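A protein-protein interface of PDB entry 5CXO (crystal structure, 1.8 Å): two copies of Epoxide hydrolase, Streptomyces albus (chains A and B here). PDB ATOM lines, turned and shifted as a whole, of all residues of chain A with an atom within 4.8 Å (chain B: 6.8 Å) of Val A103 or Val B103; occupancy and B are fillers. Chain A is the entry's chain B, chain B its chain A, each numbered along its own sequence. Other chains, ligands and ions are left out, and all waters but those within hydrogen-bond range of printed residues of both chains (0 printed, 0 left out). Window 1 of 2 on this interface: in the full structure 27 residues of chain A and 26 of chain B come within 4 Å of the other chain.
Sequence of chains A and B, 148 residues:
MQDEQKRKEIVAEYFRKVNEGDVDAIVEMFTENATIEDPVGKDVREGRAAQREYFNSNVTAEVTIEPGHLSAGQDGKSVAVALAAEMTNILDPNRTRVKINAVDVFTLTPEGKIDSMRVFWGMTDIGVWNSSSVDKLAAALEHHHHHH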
ATOM      1  N   SER A  71     -25.913   5.095  -1.615  1.00  0.00           N
ATOM      2  CA  SER A  71     -26.978   4.960  -0.574  1.00  0.00           C
ATOM      3  C   SER A  71     -28.282   4.520  -1.229  1.00  0.00           C
ATOM      4  O   SER A  71     -28.566   4.933  -2.334  1.00  0.00           O
ATOM      5  CB  SER A  71     -27.227   6.300   0.075  1.00  0.00           C
ATOM      6  OG  SER A  71     -26.034   6.665   0.836  1.00  0.00           O
ATOM      7  N   ALA A  80     -28.885   6.824  -4.214  1.00  0.00           N
ATOM      8  CA  ALA A  80     -28.443   8.194  -4.368  1.00  0.00           C
ATOM      9  C   ALA A  80     -26.928   8.162  -4.063  1.00  0.00           C
ATOM     10  O   ALA A  80     -26.553   7.422  -3.204  1.00  0.00           O
ATOM     11  CB  ALA A  80     -29.140   9.194  -3.351  1.00  0.00           C
ATOM     12  N   VAL A  81     -26.150   8.960  -4.794  1.00  0.00           N
ATOM     13  CA  VAL A  81     -24.663   8.842  -4.694  1.00  0.00           C
ATOM     14  C   VAL A  81     -23.993  10.105  -5.058  1.00  0.00           C
ATOM     15  O   VAL A  81     -24.316  10.746  -6.007  1.00  0.00           O
ATOM     16  CB  VAL A  81     -24.214   7.659  -5.604  1.00  0.00           C
ATOM     17  CG1 VAL A  81     -24.788   7.750  -7.020  1.00  0.00           C
ATOM     18  CG2 VAL A  81     -22.693   7.559  -5.649  1.00  0.00           C
ATOM     19  N   ALA A  82     -23.025  10.551  -4.269  1.00  0.00           N
ATOM     20  CA  ALA A  82     -22.209  11.709  -4.682  1.00  0.00           C
ATOM     21  C   ALA A  82     -21.055  11.204  -5.520  1.00  0.00           C
ATOM     22  O   ALA A  82     -20.473  10.125  -5.219  1.00  0.00           O
ATOM     23  CB  ALA A  82     -21.575  12.402  -3.459  1.00  0.00           C
ATOM     24  N   ASN A 101     -18.511  18.229  -9.077  1.00  0.00           N
ATOM     25  CA  ASN A 101     -18.956  17.386  -7.931  1.00  0.00           C
ATOM     26  C   ASN A 101     -20.478  17.437  -7.897  1.00  0.00           C
ATOM     27  O   ASN A 101     -21.074  18.477  -7.530  1.00  0.00           O
ATOM     28  CB  ASN A 101     -18.374  17.974  -6.630  1.00  0.00           C
ATOM     29  CG  ASN A 101     -16.927  17.504  -6.438  1.00  0.00           C
ATOM     30  OD1 ASN A 101     -16.017  18.235  -6.768  1.00  0.00           O
ATOM     31  ND2 ASN A 101     -16.721  16.284  -5.952  1.00  0.00           N
ATOM     32  N   ALA A 102     -21.062  16.292  -8.162  1.00  0.00           N
ATOM     33  CA  ALA A 102     -22.505  16.177  -8.377  1.00  0.00           C
ATOM     34  C   ALA A 102     -23.088  15.133  -7.439  1.00  0.00           C
ATOM     35  O   ALA A 102     -22.384  14.236  -6.928  1.00  0.00           O
ATOM     36  CB  ALA A 102     -22.690  15.727  -9.813  1.00  0.00           C
ATOM     37  N   VAL A 103     -24.407  15.252  -7.181  1.00  0.00           N
ATOM     38  CA  VAL A 103     -25.155  14.078  -6.674  1.00  0.00           C
ATOM     39  C   VAL A 103     -26.133  13.432  -7.642  1.00  0.00           C
ATOM     40  O   VAL A 103     -26.843  14.183  -8.263  1.00  0.00           O
ATOM     41  CB  VAL A 103     -25.905  14.477  -5.358  1.00  0.00           C
ATOM     42  CG1 VAL A 103     -26.637  13.259  -4.853  1.00  0.00           C
ATOM     43  CG2 VAL A 103     -24.827  14.900  -4.340  1.00  0.00           C
ATOM     44  N   ASP A 104     -26.041  12.131  -7.856  1.00  0.00           N
ATOM     45  CA  ASP A 104     -27.035  11.445  -8.736  1.00  0.00           C
ATOM     46  C   ASP A 104     -28.100  10.867  -7.846  1.00  0.00           C
ATOM     47  O   ASP A 104     -27.800  10.184  -6.882  1.00  0.00           O
ATOM     48  CB  ASP A 104     -26.394  10.327  -9.583  1.00  0.00           C
ATOM     49  CG  ASP A 104     -25.673  10.838 -10.739  1.00  0.00           C
ATOM     50  OD1 ASP A 104     -25.560  12.050 -10.917  1.00  0.00           O
ATOM     51  OD2 ASP A 104     -25.211   9.990 -11.525  1.00  0.00           O
ATOM     52  N   VAL A 105     -29.381  10.995  -8.258  1.00  0.00           N
ATOM     53  CA  VAL A 105     -30.445  10.158  -7.667  1.00  0.00           C
ATOM     54  C   VAL A 105     -31.136   9.315  -8.797  1.00  0.00           C
ATOM     55  O   VAL A 105     -31.582   9.921  -9.788  1.00  0.00           O
ATOM     56  CB  VAL A 105     -31.508  11.040  -6.956  1.00  0.00           C
ATOM     57  CG1 VAL A 105     -32.649  10.196  -6.389  1.00  0.00           C
ATOM     58  CG2 VAL A 105     -30.927  11.893  -5.803  1.00  0.00           C
ATOM     59  N   ARG A 118     -31.715  12.226 -11.764  1.00  0.00           N
ATOM     60  CA  ARG A 118     -31.606  13.645 -11.539  1.00  0.00           C
ATOM     61  C   ARG A 118     -30.218  13.834 -11.023  1.00  0.00           C
ATOM     62  O   ARG A 118     -29.795  13.059 -10.154  1.00  0.00           O
ATOM     63  CB  ARG A 118     -32.583  14.036 -10.454  1.00  0.00           C
ATOM     64  CG  ARG A 118     -33.861  13.251 -10.752  1.00  0.00           C
ATOM     65  CD  ARG A 118     -35.057  14.115 -10.563  1.00  0.00           C
ATOM     66  NE  ARG A 118     -34.993  14.792  -9.297  1.00  0.00           N
ATOM     67  CZ  ARG A 118     -35.265  16.070  -9.155  1.00  0.00           C
ATOM     68  NH1 ARG A 118     -35.660  16.762 -10.218  1.00  0.00           N
ATOM     69  NH2 ARG A 118     -35.142  16.650  -7.962  1.00  0.00           N
ATOM     70  N   VAL A 119     -29.528  14.748 -11.648  1.00  0.00           N
ATOM     71  CA  VAL A 119     -28.103  14.939 -11.391  1.00  0.00           C
ATOM     72  C   VAL A 119     -28.066  16.360 -10.811  1.00  0.00           C
ATOM     73  O   VAL A 119     -28.368  17.336 -11.505  1.00  0.00           O
ATOM     74  CB  VAL A 119     -27.284  14.832 -12.686  1.00  0.00           C
ATOM     75  CG1 VAL A 119     -25.773  14.979 -12.435  1.00  0.00           C
ATOM     76  CG2 VAL A 119     -27.582  13.535 -13.481  1.00  0.00           C
ATOM     77  N   PHE A 120     -27.689  16.511  -9.536  1.00  0.00           N
ATOM     78  CA  PHE A 120     -27.569  17.771  -8.959  1.00  0.00           C
ATOM     79  C   PHE A 120     -26.164  18.309  -9.093  1.00  0.00           C
ATOM     80  O   PHE A 120     -25.210  17.718  -8.560  1.00  0.00           O
ATOM     81  CB  PHE A 120     -27.898  17.703  -7.441  1.00  0.00           C
ATOM     82  CG  PHE A 120     -29.292  17.333  -7.144  1.00  0.00           C
ATOM     83  CD1 PHE A 120     -29.660  16.022  -7.168  1.00  0.00           C
ATOM     84  CD2 PHE A 120     -30.191  18.296  -6.732  1.00  0.00           C
ATOM     85  CE1 PHE A 120     -30.977  15.621  -6.909  1.00  0.00           C
ATOM     86  CE2 PHE A 120     -31.529  17.932  -6.432  1.00  0.00           C
ATOM     87  CZ  PHE A 120     -31.910  16.583  -6.562  1.00  0.00           C
ATOM     88  N   VAL B  40     -36.293   8.079   3.025  1.00  0.00           N
ATOM     89  CA  VAL B  40     -37.081   8.070   1.801  1.00  0.00           C
ATOM     90  C   VAL B  40     -37.847   6.758   1.646  1.00  0.00           C
ATOM     91  O   VAL B  40     -37.292   5.648   1.896  1.00  0.00           O
ATOM     92  CB  VAL B  40     -36.190   8.303   0.606  1.00  0.00           C
ATOM     93  CG1 VAL B  40     -36.888   7.828  -0.661  1.00  0.00           C
ATOM     94  CG2 VAL B  40     -35.717   9.787   0.534  1.00  0.00           C
ATOM     95  N   HIS B  69     -19.176  17.019   0.051  1.00  0.00           N
ATOM     96  CA  HIS B  69     -19.358  18.178  -0.814  1.00  0.00           C
ATOM     97  C   HIS B  69     -20.837  18.554  -0.988  1.00  0.00           C
ATOM     98  O   HIS B  69     -21.695  17.706  -1.127  1.00  0.00           O
ATOM     99  CB  HIS B  69     -18.809  17.869  -2.224  1.00  0.00           C
ATOM    100  CG  HIS B  69     -18.977  18.986  -3.159  1.00  0.00           C
ATOM    101  ND1 HIS B  69     -18.012  19.934  -3.322  1.00  0.00           N
ATOM    102  CD2 HIS B  69     -20.021  19.369  -3.931  1.00  0.00           C
ATOM    103  CE1 HIS B  69     -18.436  20.864  -4.176  1.00  0.00           C
ATOM    104  NE2 HIS B  69     -19.636  20.525  -4.592  1.00  0.00           N
ATOM    105  N   LEU B  70     -21.129  19.835  -0.758  1.00  0.00           N
ATOM    106  CA  LEU B  70     -22.513  20.279  -0.988  1.00  0.00           C
ATOM    107  C   LEU B  70     -22.671  20.662  -2.461  1.00  0.00           C
ATOM    108  O   LEU B  70     -22.061  21.681  -2.945  1.00  0.00           O
ATOM    109  CB  LEU B  70     -22.755  21.515  -0.072  1.00  0.00           C
ATOM    110  CG  LEU B  70     -22.911  21.364   1.499  1.00  0.00           C
ATOM    111  CD1 LEU B  70     -21.812  20.678   2.282  1.00  0.00           C
ATOM    112  CD2 LEU B  70     -23.063  22.758   2.147  1.00  0.00           C
ATOM    113  N   SER B  71     -23.523  19.916  -3.146  1.00  0.00           N
ATOM    114  CA  SER B  71     -23.843  20.171  -4.562  1.00  0.00           C
ATOM    115  C   SER B  71     -25.095  21.014  -4.622  1.00  0.00           C
ATOM    116  O   SER B  71     -26.108  20.665  -4.025  1.00  0.00           O
ATOM    117  CB  SER B  71     -24.023  18.869  -5.334  1.00  0.00           C
ATOM    118  OG  SER B  71     -22.786  18.121  -5.472  1.00  0.00           O
ATOM    119  N   VAL B  79     -30.171  21.567  -2.711  1.00  0.00           N
ATOM    120  CA  VAL B  79     -28.757  21.268  -2.345  1.00  0.00           C
ATOM    121  C   VAL B  79     -28.778  19.780  -2.111  1.00  0.00           C
ATOM    122  O   VAL B  79     -29.718  19.250  -1.452  1.00  0.00           O
ATOM    123  CB  VAL B  79     -28.346  21.984  -1.033  1.00  0.00           C
ATOM    124  CG1 VAL B  79     -26.962  21.494  -0.626  1.00  0.00           C
ATOM    125  CG2 VAL B  79     -28.302  23.498  -1.180  1.00  0.00           C
ATOM    126  N   ALA B  80     -27.746  19.047  -2.646  1.00  0.00           N
ATOM    127  CA  ALA B  80     -27.775  17.617  -2.381  1.00  0.00           C
ATOM    128  C   ALA B  80     -26.357  17.266  -1.854  1.00  0.00           C
ATOM    129  O   ALA B  80     -25.402  17.923  -2.281  1.00  0.00           O
ATOM    130  CB  ALA B  80     -28.049  16.833  -3.633  1.00  0.00           C
ATOM    131  N   VAL B  81     -26.289  16.310  -0.904  1.00  0.00           N
ATOM    132  CA  VAL B  81     -24.987  16.157  -0.222  1.00  0.00           C
ATOM    133  C   VAL B  81     -24.994  14.781   0.405  1.00  0.00           C
ATOM    134  O   VAL B  81     -25.919  14.375   1.141  1.00  0.00           O
ATOM    135  CB  VAL B  81     -24.764  17.246   0.863  1.00  0.00           C
ATOM    136  CG1 VAL B  81     -26.000  17.390   1.779  1.00  0.00           C
ATOM    137  CG2 VAL B  81     -23.514  16.976   1.745  1.00  0.00           C
ATOM    138  N   ALA B  82     -23.923  14.049   0.115  1.00  0.00           N
ATOM    139  CA  ALA B  82     -23.697  12.803   0.874  1.00  0.00           C
ATOM    140  C   ALA B  82     -23.048  13.111   2.247  1.00  0.00           C
ATOM    141  O   ALA B  82     -22.316  14.051   2.383  1.00  0.00           O
ATOM    142  CB  ALA B  82     -22.721  11.924   0.023  1.00  0.00           C
ATOM    143  N   LEU B  83     -23.401  12.328   3.255  1.00  0.00           N
ATOM    144  CA  LEU B  83     -22.956  12.549   4.584  1.00  0.00           C
ATOM    145  C   LEU B  83     -22.655  11.258   5.314  1.00  0.00           C
ATOM    146  O   LEU B  83     -23.231  10.195   5.013  1.00  0.00           O
ATOM    147  CB  LEU B  83     -23.927  13.394   5.315  1.00  0.00           C
ATOM    148  CG  LEU B  83     -25.298  12.811   5.418  1.00  0.00           C
ATOM    149  CD1 LEU B  83     -25.360  12.134   6.769  1.00  0.00           C
ATOM    150  CD2 LEU B  83     -26.197  14.010   5.334  1.00  0.00           C
ATOM    151  N   ASN B 101     -24.231   5.878   6.153  1.00  0.00           N
ATOM    152  CA  ASN B 101     -23.827   6.681   4.999  1.00  0.00           C
ATOM    153  C   ASN B 101     -25.061   7.029   4.206  1.00  0.00           C
ATOM    154  O   ASN B 101     -25.623   6.172   3.544  1.00  0.00           O
ATOM    155  CB  ASN B 101     -22.837   5.835   4.162  1.00  0.00           C
ATOM    156  CG  ASN B 101     -21.390   5.824   4.731  1.00  0.00           C
ATOM    157  OD1 ASN B 101     -21.059   6.518   5.696  1.00  0.00           O
ATOM    158  ND2 ASN B 101     -20.513   4.993   4.143  1.00  0.00           N
ATOM    159  N   ALA B 102     -25.473   8.309   4.234  1.00  0.00           N
ATOM    160  CA  ALA B 102     -26.735   8.750   3.676  1.00  0.00           C
ATOM    161  C   ALA B 102     -26.537   9.827   2.617  1.00  0.00           C
ATOM    162  O   ALA B 102     -25.413  10.381   2.450  1.00  0.00           O
ATOM    163  CB  ALA B 102     -27.612   9.403   4.776  1.00  0.00           C
ATOM    164  N   VAL B 103     -27.614  10.132   1.856  1.00  0.00           N
ATOM    165  CA  VAL B 103     -27.567  11.359   0.994  1.00  0.00           C
ATOM    166  C   VAL B 103     -28.790  12.184   1.340  1.00  0.00           C
ATOM    167  O   VAL B 103     -29.847  11.590   1.461  1.00  0.00           O
ATOM    168  CB  VAL B 103     -27.683  11.017  -0.500  1.00  0.00           C
ATOM    169  CG1 VAL B 103     -27.665  12.269  -1.277  1.00  0.00           C
ATOM    170  CG2 VAL B 103     -26.470  10.192  -0.951  1.00  0.00           C
ATOM    171  N   ASP B 104     -28.608  13.495   1.539  1.00  0.00           N
ATOM    172  CA  ASP B 104     -29.721  14.452   1.950  1.00  0.00           C
ATOM    173  C   ASP B 104     -29.963  15.314   0.772  1.00  0.00           C
ATOM    174  O   ASP B 104     -29.023  15.807   0.095  1.00  0.00           O
ATOM    175  CB  ASP B 104     -29.228  15.347   3.105  1.00  0.00           C
ATOM    176  CG  ASP B 104     -29.453  14.798   4.492  1.00  0.00           C
ATOM    177  OD1 ASP B 104     -29.746  13.613   4.664  1.00  0.00           O
ATOM    178  OD2 ASP B 104     -29.183  15.524   5.492  1.00  0.00           O
ATOM    179  N   VAL B 105     -31.235  15.500   0.419  1.00  0.00           N
ATOM    180  CA  VAL B 105     -31.497  16.524  -0.580  1.00  0.00           C
ATOM    181  C   VAL B 105     -32.450  17.544   0.107  1.00  0.00           C
ATOM    182  O   VAL B 105     -33.447  17.116   0.640  1.00  0.00           O
ATOM    183  CB  VAL B 105     -32.246  15.914  -1.795  1.00  0.00           C
ATOM    184  CG1 VAL B 105     -32.501  17.044  -2.800  1.00  0.00           C
ATOM    185  CG2 VAL B 105     -31.412  14.817  -2.500  1.00  0.00           C
ATOM    186  N   ARG B 118     -35.065  15.377   2.206  1.00  0.00           N
ATOM    187  CA  ARG B 118     -35.330  13.986   1.919  1.00  0.00           C
ATOM    188  C   ARG B 118     -34.017  13.261   2.285  1.00  0.00           C
ATOM    189  O   ARG B 118     -32.974  13.794   1.965  1.00  0.00           O
ATOM    190  CB  ARG B 118     -35.648  13.744   0.476  1.00  0.00           C
ATOM    191  CG  ARG B 118     -36.912  14.502   0.089  1.00  0.00           C
ATOM    192  CD  ARG B 118     -37.824  13.585  -0.677  1.00  0.00           C
ATOM    193  NE  ARG B 118     -37.347  13.185  -1.968  1.00  0.00           N
ATOM    194  CZ  ARG B 118     -37.610  11.972  -2.453  1.00  0.00           C
ATOM    195  NH1 ARG B 118     -38.428  11.112  -1.817  1.00  0.00           N
ATOM    196  NH2 ARG B 118     -37.131  11.629  -3.604  1.00  0.00           N
ATOM    197  N   VAL B 119     -34.105  12.158   2.996  1.00  0.00           N
ATOM    198  CA  VAL B 119     -32.874  11.490   3.456  1.00  0.00           C
ATOM    199  C   VAL B 119     -32.823  10.081   2.901  1.00  0.00           C
ATOM    200  O   VAL B 119     -33.677   9.195   3.212  1.00  0.00           O
ATOM    201  CB  VAL B 119     -32.748  11.489   4.960  1.00  0.00           C
ATOM    202  CG1 VAL B 119     -31.356  10.938   5.332  1.00  0.00           C
ATOM    203  CG2 VAL B 119     -32.989  12.927   5.540  1.00  0.00           C
ATOM    204  N   PHE B 120     -31.822   9.819   2.062  1.00  0.00           N
ATOM    205  CA  PHE B 120     -31.710   8.476   1.488  1.00  0.00           C
ATOM    206  C   PHE B 120     -30.750   7.662   2.302  1.00  0.00           C
ATOM    207  O   PHE B 120     -29.535   7.934   2.294  1.00  0.00           O
ATOM    208  CB  PHE B 120     -31.128   8.575   0.076  1.00  0.00           C
ATOM    209  CG  PHE B 120     -32.080   9.208  -0.967  1.00  0.00           C
ATOM    210  CD1 PHE B 120     -32.157  10.599  -1.092  1.00  0.00           C
ATOM    211  CD2 PHE B 120     -32.853   8.382  -1.808  1.00  0.00           C
ATOM    212  CE1 PHE B 120     -32.975  11.238  -2.031  1.00  0.00           C
ATOM    213  CE2 PHE B 120     -33.658   9.021  -2.763  1.00  0.00           C
ATOM    214  CZ  PHE B 120     -33.703  10.423  -2.869  1.00  0.00           C
ATOM    215  N   TRP B 121     -31.243   6.635   2.995  1.00  0.00           N
ATOM    216  CA  TRP B 121     -30.368   5.650   3.589  1.00  0.00           C
ATOM    217  C   TRP B 121     -31.170   4.398   3.736  1.00  0.00           C
ATOM    218  O   TRP B 121     -32.388   4.476   3.930  1.00  0.00           O
ATOM    219  CB  TRP B 121     -29.828   6.083   4.958  1.00  0.00           C
ATOM    220  CG  TRP B 121     -30.994   6.229   6.033  1.00  0.00           C
ATOM    221  CD1 TRP B 121     -31.799   7.327   6.246  1.00  0.00           C
ATOM    222  CD2 TRP B 121     -31.480   5.201   6.914  1.00  0.00           C
ATOM    223  NE1 TRP B 121     -32.711   7.053   7.192  1.00  0.00           N
ATOM    224  CE2 TRP B 121     -32.542   5.764   7.650  1.00  0.00           C
ATOM    225  CE3 TRP B 121     -31.097   3.872   7.179  1.00  0.00           C
ATOM    226  CZ2 TRP B 121     -33.250   5.045   8.582  1.00  0.00           C
ATOM    227  CZ3 TRP B 121     -31.791   3.147   8.137  1.00  0.00           C
ATOM    228  CH2 TRP B 121     -32.849   3.735   8.857  1.00  0.00           C
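The backbone carbonyl oxygen (O) of Asn B101 is in hydrogen-bond range of the side-chain hydroxyl (OG) of Ser A71.
The backbone carbonyl oxygen (O) of Asn A101 lies within hydrogen-bond range of the side-chain hydroxyl (OG) of Ser B71, at 2.7 Å.
O of Val B105 lies within hydrogen-bond range of N of Arg B118, at 2.8 Å.
The backbone carbonyl oxygen (O) of Val B103 sits at hydrogen-bond distance from the backbone NH (N) of Phe B120, at 2.7 Å.
The backbone NH (N) of Ala A80 lies within hydrogen-bond range of the backbone carbonyl oxygen (O) of Ser A71 (2.7 Å).
O of Ala B102 sits at hydrogen-bond distance from N of Leu B83.
The backbone carbonyl oxygen (O) of Val A103 sits at hydrogen-bond distance from the backbone NH (N) of Phe A120, at 2.8 Å.
N of Val A105 lies within hydrogen-bond range of O of Arg A118 (2.8 Å).
Among the printed residues, merely in contact across the chains: Ser A71 with Ala B102 (3.6 Å), Ser A71 with Val B103 (3.9 Å), Ser A71 with Phe B120 (3.6 Å), Ala A80 with Val B103 (3.6 Å), Ala A80 with Phe B120 (3.8 Å), Ala A82 with Ala B82 (3.7 Å), Asn A101 with His B69 (3.5 Å), Ala A102 with Ser B71 (3.5 Å), Val A103 with Ser B71 (3.7 Å), Val A103 with Ala B80 (3.6 Å), Val A103 with Val B81 (3.99 Å), Val A103 with Val B103 (3.9 Å), Val A105 with Phe B120 (3.7 Å), Phe A120 with Ser B71 (3.6 Å), Phe A120 with Ala B80 (3.8 Å) and Phe A120 with Val B105 (3.8 Å).
Of the printed residues of chain B, Val A103 touches Ser B71, Ala B80, Val B81 and Val B103.
Of the printed residues of chain A, Val B81 touches Val A103 (3.99 Å).
Printed residues of chain A within 4 Å of Ala B102: Ser A71.
Of chain A, only Ser A71 (3.9 Å), Ala A80 (3.6 Å) and Val A103 (3.9 Å) come within 4 Å of Val B103.
The nearest residue of chain A that does not touch Val B103 is Val A81 (4.05 Å).
The nearest printed residue of chain A that does not touch Asn B101 is Ala A80 (6.9 Å).
Of the 18 printed residues of chain B, 10 touch a printed residue of chain A.
Printed residues of chain B that touch a printed residue of chain A: His B69, Ser B71, Ala B80, Val B81, Ala B82, Asn B101, Ala B102, Val B103, Val B105 and Phe B120.
Hydrophobic or aromatic side chains of chain B that line the printed part of chain A: His B69, Ala B80, Ala B82, Val B103, Val B105 and Phe B120.
Among the printed residues, 18 pairs touch across the chains.
Among the printed residues, no Asp or Glu carboxylate lies within 4 Å of a Lys or Arg side-chain nitrogen of the other chain.
Ser A71 touches Ala B102, and with the chains exchanged Ala A102 touches Ser B71.
Ser A71 touches Val B103, and with the chains exchanged Val A103 touches Ser B71.
Ala A80 touches Phe B120, and with the chains exchanged Phe A120 touches Ala B80.
Ala B82 touches its own counterpart, Ala A82.
12 positions are printed for both chains.
Of the 18 pairs that touch across the chains among the printed residues, 16 have their exchanged pair printed and touching as well.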
